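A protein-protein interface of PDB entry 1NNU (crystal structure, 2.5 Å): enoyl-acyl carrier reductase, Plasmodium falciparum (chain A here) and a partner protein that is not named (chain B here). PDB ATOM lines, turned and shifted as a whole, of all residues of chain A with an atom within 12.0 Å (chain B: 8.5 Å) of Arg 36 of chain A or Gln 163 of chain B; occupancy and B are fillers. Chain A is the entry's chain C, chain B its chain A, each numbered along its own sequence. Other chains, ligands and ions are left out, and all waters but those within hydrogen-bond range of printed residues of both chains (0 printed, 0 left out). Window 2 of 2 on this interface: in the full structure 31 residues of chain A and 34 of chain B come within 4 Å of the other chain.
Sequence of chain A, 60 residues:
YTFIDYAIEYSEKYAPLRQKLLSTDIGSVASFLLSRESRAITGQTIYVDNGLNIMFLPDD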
ATOM      1  N   SER A  28      35.337 -28.813  22.847  1.00  0.00           N
ATOM      2  CA  SER A  28      34.969 -27.449  22.505  1.00  0.00           C
ATOM      3  C   SER A  28      34.353 -27.389  21.115  1.00  0.00           C
ATOM      4  O   SER A  28      33.495 -26.547  20.850  1.00  0.00           O
ATOM      5  CB  SER A  28      36.184 -26.529  22.585  1.00  0.00           C
ATOM      6  OG  SER A  28      37.141 -26.908  21.625  1.00  0.00           O
ATOM      7  N   VAL A  29      34.780 -28.278  20.226  1.00  0.00           N
ATOM      8  CA  VAL A  29      34.214 -28.284  18.885  1.00  0.00           C
ATOM      9  C   VAL A  29      32.797 -28.866  18.953  1.00  0.00           C
ATOM     10  O   VAL A  29      31.872 -28.352  18.320  1.00  0.00           O
ATOM     11  CB  VAL A  29      35.079 -29.098  17.892  1.00  0.00           C
ATOM     12  CG1 VAL A  29      34.417 -29.102  16.530  1.00  0.00           C
ATOM     13  CG2 VAL A  29      36.471 -28.483  17.772  1.00  0.00           C
ATOM     14  N   ALA A  30      32.629 -29.929  19.734  1.00  0.00           N
ATOM     15  CA  ALA A  30      31.320 -30.544  19.900  1.00  0.00           C
ATOM     16  C   ALA A  30      30.365 -29.460  20.410  1.00  0.00           C
ATOM     17  O   ALA A  30      29.298 -29.206  19.836  1.00  0.00           O
ATOM     18  CB  ALA A  30      31.407 -31.678  20.910  1.00  0.00           C
ATOM     19  N   SER A  31      30.784 -28.818  21.495  1.00  0.00           N
ATOM     20  CA  SER A  31      30.018 -27.761  22.130  1.00  0.00           C
ATOM     21  C   SER A  31      29.538 -26.718  21.125  1.00  0.00           C
ATOM     22  O   SER A  31      28.395 -26.269  21.179  1.00  0.00           O
ATOM     23  CB  SER A  31      30.873 -27.101  23.204  1.00  0.00           C
ATOM     24  OG  SER A  31      30.125 -26.136  23.906  1.00  0.00           O
ATOM     25  N   PHE A  32      30.412 -26.331  20.204  1.00  0.00           N
ATOM     26  CA  PHE A  32      30.051 -25.346  19.189  1.00  0.00           C
ATOM     27  C   PHE A  32      29.032 -25.894  18.175  1.00  0.00           C
ATOM     28  O   PHE A  32      28.106 -25.184  17.778  1.00  0.00           O
ATOM     29  CB  PHE A  32      31.302 -24.856  18.447  1.00  0.00           C
ATOM     30  CG  PHE A  32      30.993 -24.147  17.158  1.00  0.00           C
ATOM     31  CD1 PHE A  32      30.446 -22.873  17.164  1.00  0.00           C
ATOM     32  CD2 PHE A  32      31.189 -24.785  15.936  1.00  0.00           C
ATOM     33  CE1 PHE A  32      30.091 -22.244  15.970  1.00  0.00           C
ATOM     34  CE2 PHE A  32      30.840 -24.167  14.741  1.00  0.00           C
ATOM     35  CZ  PHE A  32      30.288 -22.894  14.759  1.00  0.00           C
ATOM     36  N   LEU A  33      29.207 -27.145  17.755  1.00  0.00           N
ATOM     37  CA  LEU A  33      28.288 -27.756  16.794  1.00  0.00           C
ATOM     38  C   LEU A  33      26.928 -28.036  17.420  1.00  0.00           C
ATOM     39  O   LEU A  33      25.925 -28.164  16.725  1.00  0.00           O
ATOM     40  CB  LEU A  33      28.861 -29.068  16.251  1.00  0.00           C
ATOM     41  CG  LEU A  33      30.023 -28.967  15.260  1.00  0.00           C
ATOM     42  CD1 LEU A  33      30.539 -30.364  14.926  1.00  0.00           C
ATOM     43  CD2 LEU A  33      29.553 -28.245  14.003  1.00  0.00           C
ATOM     44  N   LEU A  34      26.899 -28.136  18.741  1.00  0.00           N
ATOM     45  CA  LEU A  34      25.660 -28.416  19.435  1.00  0.00           C
ATOM     46  C   LEU A  34      24.869 -27.149  19.749  1.00  0.00           C
ATOM     47  O   LEU A  34      23.695 -27.221  20.110  1.00  0.00           O
ATOM     48  CB  LEU A  34      25.958 -29.198  20.719  1.00  0.00           C
ATOM     49  CG  LEU A  34      26.454 -30.637  20.529  1.00  0.00           C
ATOM     50  CD1 LEU A  34      26.797 -31.267  21.874  1.00  0.00           C
ATOM     51  CD2 LEU A  34      25.376 -31.444  19.843  1.00  0.00           C
ATOM     52  N   SER A  35      25.509 -25.992  19.590  1.00  0.00           N
ATOM     53  CA  SER A  35      24.859 -24.722  19.878  1.00  0.00           C
ATOM     54  C   SER A  35      24.247 -24.109  18.630  1.00  0.00           C
ATOM     55  O   SER A  35      24.500 -24.559  17.516  1.00  0.00           O
ATOM     56  CB  SER A  35      25.855 -23.731  20.498  1.00  0.00           C
ATOM     57  OG  SER A  35      26.747 -23.204  19.531  1.00  0.00           O
ATOM     58  N   ARG A  36      23.434 -23.079  18.833  1.00  0.00           N
ATOM     59  CA  ARG A  36      22.772 -22.386  17.739  1.00  0.00           C
ATOM     60  C   ARG A  36      23.764 -21.632  16.864  1.00  0.00           C
ATOM     61  O   ARG A  36      23.437 -21.224  15.756  1.00  0.00           O
ATOM     62  CB  ARG A  36      21.729 -21.417  18.303  1.00  0.00           C
ATOM     63  CG  ARG A  36      20.438 -22.093  18.760  1.00  0.00           C
ATOM     64  CD  ARG A  36      19.309 -21.868  17.754  1.00  0.00           C
ATOM     65  NE  ARG A  36      18.776 -20.505  17.832  1.00  0.00           N
ATOM     66  CZ  ARG A  36      17.927 -19.974  16.953  1.00  0.00           C
ATOM     67  NH1 ARG A  36      17.507 -20.688  15.914  1.00  0.00           N
ATOM     68  NH2 ARG A  36      17.488 -18.731  17.121  1.00  0.00           N
ATOM     69  N   GLU A  37      24.978 -21.454  17.369  1.00  0.00           N
ATOM     70  CA  GLU A  37      26.019 -20.746  16.636  1.00  0.00           C
ATOM     71  C   GLU A  37      26.268 -21.401  15.291  1.00  0.00           C
ATOM     72  O   GLU A  37      26.662 -20.739  14.336  1.00  0.00           O
ATOM     73  CB  GLU A  37      27.324 -20.753  17.431  1.00  0.00           C
ATOM     74  CG  GLU A  37      27.192 -20.265  18.855  1.00  0.00           C
ATOM     75  CD  GLU A  37      27.068 -18.761  18.941  1.00  0.00           C
ATOM     76  OE1 GLU A  37      26.205 -18.188  18.239  1.00  0.00           O
ATOM     77  OE2 GLU A  37      27.837 -18.152  19.718  1.00  0.00           O
ATOM     78  N   SER A  38      26.040 -22.707  15.221  1.00  0.00           N
ATOM     79  CA  SER A  38      26.271 -23.451  13.992  1.00  0.00           C
ATOM     80  C   SER A  38      24.977 -23.847  13.274  1.00  0.00           C
ATOM     81  O   SER A  38      24.898 -24.916  12.668  1.00  0.00           O
ATOM     82  CB  SER A  38      27.087 -24.703  14.313  1.00  0.00           C
ATOM     83  OG  SER A  38      26.390 -25.535  15.226  1.00  0.00           O
ATOM     84  N   ARG A  39      23.977 -22.975  13.331  1.00  0.00           N
ATOM     85  CA  ARG A  39      22.684 -23.254  12.718  1.00  0.00           C
ATOM     86  C   ARG A  39      22.732 -23.557  11.223  1.00  0.00           C
ATOM     87  O   ARG A  39      21.799 -24.150  10.691  1.00  0.00           O
ATOM     88  CB  ARG A  39      21.718 -22.087  12.967  1.00  0.00           C
ATOM     89  CG  ARG A  39      22.115 -20.788  12.296  1.00  0.00           C
ATOM     90  CD  ARG A  39      21.234 -19.632  12.743  1.00  0.00           C
ATOM     91  NE  ARG A  39      19.862 -19.729  12.247  1.00  0.00           N
ATOM     92  CZ  ARG A  39      19.417 -19.173  11.120  1.00  0.00           C
ATOM     93  NH1 ARG A  39      20.232 -18.465  10.349  1.00  0.00           N
ATOM     94  NH2 ARG A  39      18.145 -19.313  10.769  1.00  0.00           N
ATOM     95  N   ALA A  40      23.809 -23.168  10.547  1.00  0.00           N
ATOM     96  CA  ALA A  40      23.910 -23.395   9.105  1.00  0.00           C
ATOM     97  C   ALA A  40      24.758 -24.601   8.723  1.00  0.00           C
ATOM     98  O   ALA A  40      25.058 -24.806   7.551  1.00  0.00           O
ATOM     99  CB  ALA A  40      24.460 -22.148   8.423  1.00  0.00           C
ATOM    100  N   ILE A  41      25.153 -25.391   9.711  1.00  0.00           N
ATOM    101  CA  ILE A  41      25.976 -26.560   9.448  1.00  0.00           C
ATOM    102  C   ILE A  41      25.206 -27.820   9.781  1.00  0.00           C
ATOM    103  O   ILE A  41      24.633 -27.939  10.864  1.00  0.00           O
ATOM    104  CB  ILE A  41      27.261 -26.569  10.308  1.00  0.00           C
ATOM    105  CG1 ILE A  41      28.071 -25.291  10.082  1.00  0.00           C
ATOM    106  CG2 ILE A  41      28.116 -27.771   9.945  1.00  0.00           C
ATOM    107  CD1 ILE A  41      29.352 -25.238  10.890  1.00  0.00           C
ATOM    108  N   THR A  42      25.174 -28.756   8.842  1.00  0.00           N
ATOM    109  CA  THR A  42      24.504 -30.024   9.088  1.00  0.00           C
ATOM    110  C   THR A  42      24.925 -31.053   8.059  1.00  0.00           C
ATOM    111  O   THR A  42      25.216 -30.709   6.920  1.00  0.00           O
ATOM    112  CB  THR A  42      22.970 -29.879   9.083  1.00  0.00           C
ATOM    113  OG1 THR A  42      22.391 -31.115   9.509  1.00  0.00           O
ATOM    114  CG2 THR A  42      22.457 -29.542   7.697  1.00  0.00           C
ATOM    115  N   ASP B   2      19.510 -25.733  28.539  1.00  0.00           N
ATOM    116  CA  ASP B   2      19.955 -26.763  27.613  1.00  0.00           C
ATOM    117  C   ASP B   2      20.211 -28.069  28.371  1.00  0.00           C
ATOM    118  O   ASP B   2      20.828 -28.073  29.443  1.00  0.00           O
ATOM    119  CB  ASP B   2      21.247 -26.325  26.911  1.00  0.00           C
ATOM    120  CG  ASP B   2      21.111 -24.989  26.200  1.00  0.00           C
ATOM    121  OD1 ASP B   2      20.121 -24.797  25.472  1.00  0.00           O
ATOM    122  OD2 ASP B   2      22.004 -24.131  26.355  1.00  0.00           O
ATOM    123  N   ARG B  26      29.590 -24.257  29.631  1.00  0.00           N
ATOM    124  CA  ARG B  26      28.600 -23.323  29.106  1.00  0.00           C
ATOM    125  C   ARG B  26      27.226 -23.500  29.767  1.00  0.00           C
ATOM    126  O   ARG B  26      26.193 -23.151  29.192  1.00  0.00           O
ATOM    127  CB  ARG B  26      28.477 -23.496  27.589  1.00  0.00           C
ATOM    128  CG  ARG B  26      29.797 -23.356  26.842  1.00  0.00           C
ATOM    129  CD  ARG B  26      29.600 -23.432  25.327  1.00  0.00           C
ATOM    130  NE  ARG B  26      30.864 -23.418  24.584  1.00  0.00           N
ATOM    131  CZ  ARG B  26      30.954 -23.440  23.253  1.00  0.00           C
ATOM    132  NH1 ARG B  26      29.852 -23.476  22.511  1.00  0.00           N
ATOM    133  NH2 ARG B  26      32.146 -23.433  22.661  1.00  0.00           N
ATOM    134  N   ILE B 113      14.795 -32.330  25.654  1.00  0.00           N
ATOM    135  CA  ILE B 113      16.202 -31.943  25.612  1.00  0.00           C
ATOM    136  C   ILE B 113      16.479 -31.353  24.236  1.00  0.00           C
ATOM    137  O   ILE B 113      15.665 -31.492  23.322  1.00  0.00           O
ATOM    138  CB  ILE B 113      17.139 -33.143  25.846  1.00  0.00           C
ATOM    139  CG1 ILE B 113      17.014 -34.143  24.701  1.00  0.00           C
ATOM    140  CG2 ILE B 113      16.785 -33.814  27.154  1.00  0.00           C
ATOM    141  CD1 ILE B 113      17.943 -35.328  24.824  1.00  0.00           C
ATOM    142  N   ASN B 114      17.620 -30.693  24.083  1.00  0.00           N
ATOM    143  CA  ASN B 114      17.936 -30.084  22.805  1.00  0.00           C
ATOM    144  C   ASN B 114      19.331 -30.401  22.273  1.00  0.00           C
ATOM    145  O   ASN B 114      19.753 -29.839  21.260  1.00  0.00           O
ATOM    146  CB  ASN B 114      17.730 -28.570  22.898  1.00  0.00           C
ATOM    147  CG  ASN B 114      18.592 -27.935  23.953  1.00  0.00           C
ATOM    148  OD1 ASN B 114      18.717 -28.453  25.058  1.00  0.00           O
ATOM    149  ND2 ASN B 114      19.188 -26.799  23.624  1.00  0.00           N
ATOM    150  N   MET B 115      20.033 -31.308  22.949  1.00  0.00           N
ATOM    151  CA  MET B 115      21.378 -31.712  22.540  1.00  0.00           C
ATOM    152  C   MET B 115      21.580 -33.196  22.783  1.00  0.00           C
ATOM    153  O   MET B 115      21.292 -33.704  23.860  1.00  0.00           O
ATOM    154  CB  MET B 115      22.440 -30.937  23.321  1.00  0.00           C
ATOM    155  CG  MET B 115      22.334 -29.434  23.195  1.00  0.00           C
ATOM    156  SD  MET B 115      23.663 -28.640  24.078  1.00  0.00           S
ATOM    157  CE  MET B 115      23.767 -27.081  23.212  1.00  0.00           C
ATOM    158  N   MET B 160      12.894 -34.101  21.747  1.00  0.00           N
ATOM    159  CA  MET B 160      13.796 -32.985  21.478  1.00  0.00           C
ATOM    160  C   MET B 160      13.035 -31.784  20.934  1.00  0.00           C
ATOM    161  O   MET B 160      12.008 -31.938  20.280  1.00  0.00           O
ATOM    162  CB  MET B 160      14.872 -33.397  20.472  1.00  0.00           C
ATOM    163  CG  MET B 160      15.821 -34.452  20.989  1.00  0.00           C
ATOM    164  SD  MET B 160      17.047 -34.896  19.763  1.00  0.00           S
ATOM    165  CE  MET B 160      18.262 -33.615  20.061  1.00  0.00           C
ATOM    166  N   LYS B 161      13.546 -30.588  21.205  1.00  0.00           N
ATOM    167  CA  LYS B 161      12.911 -29.369  20.724  1.00  0.00           C
ATOM    168  C   LYS B 161      13.382 -29.018  19.317  1.00  0.00           C
ATOM    169  O   LYS B 161      14.405 -29.521  18.855  1.00  0.00           O
ATOM    170  CB  LYS B 161      13.209 -28.209  21.682  1.00  0.00           C
ATOM    171  CG  LYS B 161      12.325 -28.216  22.914  1.00  0.00           C
ATOM    172  CD  LYS B 161      12.584 -27.030  23.831  1.00  0.00           C
ATOM    173  CE  LYS B 161      13.731 -27.301  24.788  1.00  0.00           C
ATOM    174  NZ  LYS B 161      13.815 -26.257  25.849  1.00  0.00           N
ATOM    175  N   PRO B 162      12.622 -28.170  18.601  1.00  0.00           N
ATOM    176  CA  PRO B 162      13.048 -27.803  17.249  1.00  0.00           C
ATOM    177  C   PRO B 162      14.396 -27.108  17.370  1.00  0.00           C
ATOM    178  O   PRO B 162      14.692 -26.507  18.402  1.00  0.00           O
ATOM    179  CB  PRO B 162      11.956 -26.839  16.789  1.00  0.00           C
ATOM    180  CG  PRO B 162      10.757 -27.293  17.546  1.00  0.00           C
ATOM    181  CD  PRO B 162      11.322 -27.556  18.920  1.00  0.00           C
ATOM    182  N   GLN B 163      15.204 -27.195  16.319  1.00  0.00           N
ATOM    183  CA  GLN B 163      16.520 -26.572  16.293  1.00  0.00           C
ATOM    184  C   GLN B 163      17.502 -27.258  17.229  1.00  0.00           C
ATOM    185  O   GLN B 163      18.487 -26.658  17.659  1.00  0.00           O
ATOM    186  CB  GLN B 163      16.419 -25.089  16.646  1.00  0.00           C
ATOM    187  CG  GLN B 163      15.374 -24.338  15.840  1.00  0.00           C
ATOM    188  CD  GLN B 163      15.385 -22.848  16.122  1.00  0.00           C
ATOM    189  OE1 GLN B 163      15.628 -22.417  17.254  1.00  0.00           O
ATOM    190  NE2 GLN B 163      15.111 -22.052  15.097  1.00  0.00           N
ATOM    191  N   SER B 164      17.230 -28.514  17.562  1.00  0.00           N
ATOM    192  CA  SER B 164      18.139 -29.252  18.417  1.00  0.00           C
ATOM    193  C   SER B 164      19.302 -29.653  17.538  1.00  0.00           C
ATOM    194  O   SER B 164      19.258 -29.478  16.320  1.00  0.00           O
ATOM    195  CB  SER B 164      17.473 -30.499  18.994  1.00  0.00           C
ATOM    196  OG  SER B 164      16.677 -30.172  20.121  1.00  0.00           O
ATOM    197  N   SER B 165      20.345 -30.184  18.156  1.00  0.00           N
ATOM    198  CA  SER B 165      21.526 -30.596  17.417  1.00  0.00           C
ATOM    199  C   SER B 165      22.047 -31.931  17.941  1.00  0.00           C
ATOM    200  O   SER B 165      21.898 -32.258  19.122  1.00  0.00           O
ATOM    201  CB  SER B 165      22.603 -29.520  17.527  1.00  0.00           C
ATOM    202  OG  SER B 165      23.661 -29.783  16.628  1.00  0.00           O
ATOM    203  N   ILE B 166      22.667 -32.694  17.049  1.00  0.00           N
ATOM    204  CA  ILE B 166      23.194 -34.011  17.379  1.00  0.00           C
ATOM    205  C   ILE B 166      24.570 -34.226  16.742  1.00  0.00           C
ATOM    206  O   ILE B 166      24.804 -33.810  15.606  1.00  0.00           O
ATOM    207  CB  ILE B 166      22.236 -35.108  16.841  1.00  0.00           C
ATOM    208  CG1 ILE B 166      20.806 -34.833  17.330  1.00  0.00           C
ATOM    209  CG2 ILE B 166      22.735 -36.484  17.253  1.00  0.00           C
ATOM    210  CD1 ILE B 166      19.717 -35.613  16.588  1.00  0.00           C
ATOM    211  N   LEU B 203      16.043 -35.390   9.310  1.00  0.00           N
ATOM    212  CA  LEU B 203      15.905 -34.599  10.522  1.00  0.00           C
ATOM    213  C   LEU B 203      15.839 -33.108  10.209  1.00  0.00           C
ATOM    214  O   LEU B 203      15.202 -32.339  10.934  1.00  0.00           O
ATOM    215  CB  LEU B 203      17.067 -34.895  11.473  1.00  0.00           C
ATOM    216  CG  LEU B 203      17.108 -36.352  11.941  1.00  0.00           C
ATOM    217  CD1 LEU B 203      18.385 -36.642  12.713  1.00  0.00           C
ATOM    218  CD2 LEU B 203      15.885 -36.626  12.802  1.00  0.00           C
ATOM    219  N   GLY B 204      16.489 -32.701   9.125  1.00  0.00           N
ATOM    220  CA  GLY B 204      16.486 -31.297   8.761  1.00  0.00           C
ATOM    221  C   GLY B 204      15.159 -30.848   8.178  1.00  0.00           C
ATOM    222  O   GLY B 204      14.617 -29.820   8.573  1.00  0.00           O
ATOM    223  N   TYR B 207      12.113 -31.998  11.098  1.00  0.00           N
ATOM    224  CA  TYR B 207      12.111 -31.436  12.443  1.00  0.00           C
ATOM    225  C   TYR B 207      12.949 -30.185  12.628  1.00  0.00           C
ATOM    226  O   TYR B 207      12.924 -29.566  13.689  1.00  0.00           O
ATOM    227  CB  TYR B 207      12.587 -32.504  13.419  1.00  0.00           C
ATOM    228  CG  TYR B 207      11.836 -33.806  13.293  1.00  0.00           C
ATOM    229  CD1 TYR B 207      10.563 -33.955  13.843  1.00  0.00           C
ATOM    230  CD2 TYR B 207      12.399 -34.896  12.630  1.00  0.00           C
ATOM    231  CE1 TYR B 207       9.871 -35.163  13.743  1.00  0.00           C
ATOM    232  CE2 TYR B 207      11.714 -36.108  12.520  1.00  0.00           C
ATOM    233  CZ  TYR B 207      10.453 -36.232  13.084  1.00  0.00           C
ATOM    234  OH  TYR B 207       9.781 -37.429  13.010  1.00  0.00           O
ATOM    235  N   ASN B 208      13.690 -29.814  11.595  1.00  0.00           N
ATOM    236  CA  ASN B 208      14.553 -28.648  11.662  1.00  0.00           C
ATOM    237  C   ASN B 208      15.631 -28.946  12.703  1.00  0.00           C
ATOM    238  O   ASN B 208      16.056 -28.077  13.456  1.00  0.00           O
ATOM    239  CB  ASN B 208      13.745 -27.403  12.046  1.00  0.00           C
ATOM    240  CG  ASN B 208      14.486 -26.109  11.751  1.00  0.00           C
ATOM    241  OD1 ASN B 208      14.894 -25.857  10.613  1.00  0.00           O
ATOM    242  ND2 ASN B 208      14.664 -25.275  12.778  1.00  0.00           N
ATOM    243  N   ILE B 209      16.064 -30.200  12.742  1.00  0.00           N
ATOM    244  CA  ILE B 209      17.103 -30.614  13.665  1.00  0.00           C
ATOM    245  C   ILE B 209      18.375 -30.890  12.870  1.00  0.00           C
ATOM    246  O   ILE B 209      18.327 -31.424  11.767  1.00  0.00           O
ATOM    247  CB  ILE B 209      16.682 -31.873  14.447  1.00  0.00           C
ATOM    248  CG1 ILE B 209      15.542 -31.514  15.406  1.00  0.00           C
ATOM    249  CG2 ILE B 209      17.876 -32.453  15.197  1.00  0.00           C
ATOM    250  CD1 ILE B 209      15.045 -32.668  16.263  1.00  0.00           C
ATOM    251  N   ARG B 210      19.513 -30.507  13.436  1.00  0.00           N
ATOM    252  CA  ARG B 210      20.792 -30.692  12.773  1.00  0.00           C
ATOM    253  C   ARG B 210      21.558 -31.886  13.314  1.00  0.00           C
ATOM    254  O   ARG B 210      21.427 -32.256  14.479  1.00  0.00           O
ATOM    255  CB  ARG B 210      21.647 -29.428  12.932  1.00  0.00           C
ATOM    256  CG  ARG B 210      21.009 -28.176  12.355  1.00  0.00           C
ATOM    257  CD  ARG B 210      21.919 -26.957  12.436  1.00  0.00           C
ATOM    258  NE  ARG B 210      22.228 -26.566  13.807  1.00  0.00           N
ATOM    259  CZ  ARG B 210      23.368 -26.849  14.428  1.00  0.00           C
ATOM    260  NH1 ARG B 210      24.318 -27.526  13.800  1.00  0.00           N
ATOM    261  NH2 ARG B 210      23.565 -26.447  15.676  1.00  0.00           N
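O of Ile 41 of chain A is in hydrogen-bond range of NH1 of Arg 210 of chain B, at 3.0 Å. The guanidinium group (NH2) of Arg 210 of chain B is in hydrogen-bond range of the backbone carbonyl oxygen (O) of Ser 35 of chain A (2.8 Å). NH1 of Arg 210 of chain B sits at hydrogen-bond distance from O of Ser 38 of chain A. O of Leu 33 of chain A sits at hydrogen-bond distance from OG of Ser 165 of chain B (2.8 Å). The guanidinium group of Arg 26 of chain B lies close to the side-chain hydroxyl of Ser 31 of chain A (2.9 Å). The guanidinium group (NH2) of Arg 210 of chain B sits at hydrogen-bond distance from the backbone carbonyl oxygen (O) of Leu 33 of chain A (3.1 Å). NE2 of Gln 163 of chain B lies close to NH1 of Arg 36 of chain A (2.9 Å).
The side-chain hydroxyl (OG) of Ser 165 of chain B sits at hydrogen-bond distance from the guanidinium group (NH2) of Arg 210 of chain B (3.5 Å). OG of Ser 38 of chain A sits at hydrogen-bond distance from O of Ser 35 of chain A. O of Ser 164 of chain B sits at hydrogen-bond distance from N of Arg 210 of chain B (3.1 Å). The backbone carbonyl oxygen (O) of Phe 32 of chain A lies within hydrogen-bond range of the side-chain hydroxyl (OG) of Ser 35 of chain A, 3.0 Å away. O of Asn 114 of chain B sits at hydrogen-bond distance from N of Ser 165 of chain B, at 3.2 Å. The backbone carbonyl oxygen of Arg 210 of chain B is in hydrogen-bond range of the backbone NH of Ile 166 of chain B (2.9 Å).
Among the printed residues, pairs that only touch across the chains: Ser 28 of chain A with Arg 26 of chain B, Phe 32 of chain A with Arg 26 of chain B, Leu 34 of chain A with Met 115 of chain B, Leu 34 of chain A with Ser 165 of chain B, Arg 39 of chain A with Arg 210 of chain B and Thr 42 of chain A with Arg 210 of chain B.
Of chain B, only Gln 163 comes within 4 Å of Arg 36 of chain A. Gln 163 of chain B touches just one residue of chain A: Arg 36 (2.9 Å). No residue of chain A comes within 4 Å of Pro 162 of chain B. Ser 165 of chain B touches two residues of chain A. No residue of chain A comes within 4 Å of Asn 208 of chain B. No residue of chain A comes within 4 Å of Ile 209 of chain B. Printed residues of chain B within 4 Å of Leu 33 of chain A: Ser 165 (2.8 Å) and Arg 210 (3.1 Å). Of the printed residues of chain A, Met 115 of chain B touches Leu 34. Printed residues of chain B within 4 Å of Ile 41 of chain A: Arg 210. Of the printed residues of chain B, Leu 34 of chain A touches Met 115 and Ser 165. Printed residues of chain B within 4 Å of Ser 38 of chain A: Arg 210 (2.9 Å). Asp 2 of chain B touches none of the printed residues of chain A. The nearest printed residue of chain A that does not touch Met 115 of chain B is Ser 35 of chain A (4.2 Å).
Of the 18 printed residues of chain B, 5 touch a printed residue of chain A. Hydrophobic or aromatic side chains of chain A that line the printed part of chain B: Leu 34. Along chain A the printed residues that touch a printed residue of chain B span positions 28 to 42. Among the printed residues, 13 pairs touch across the chains. Among the printed residues, no Asp or Glu carboxylate lies within 4 Å of a Lys or Arg side-chain nitrogen of the other chain.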
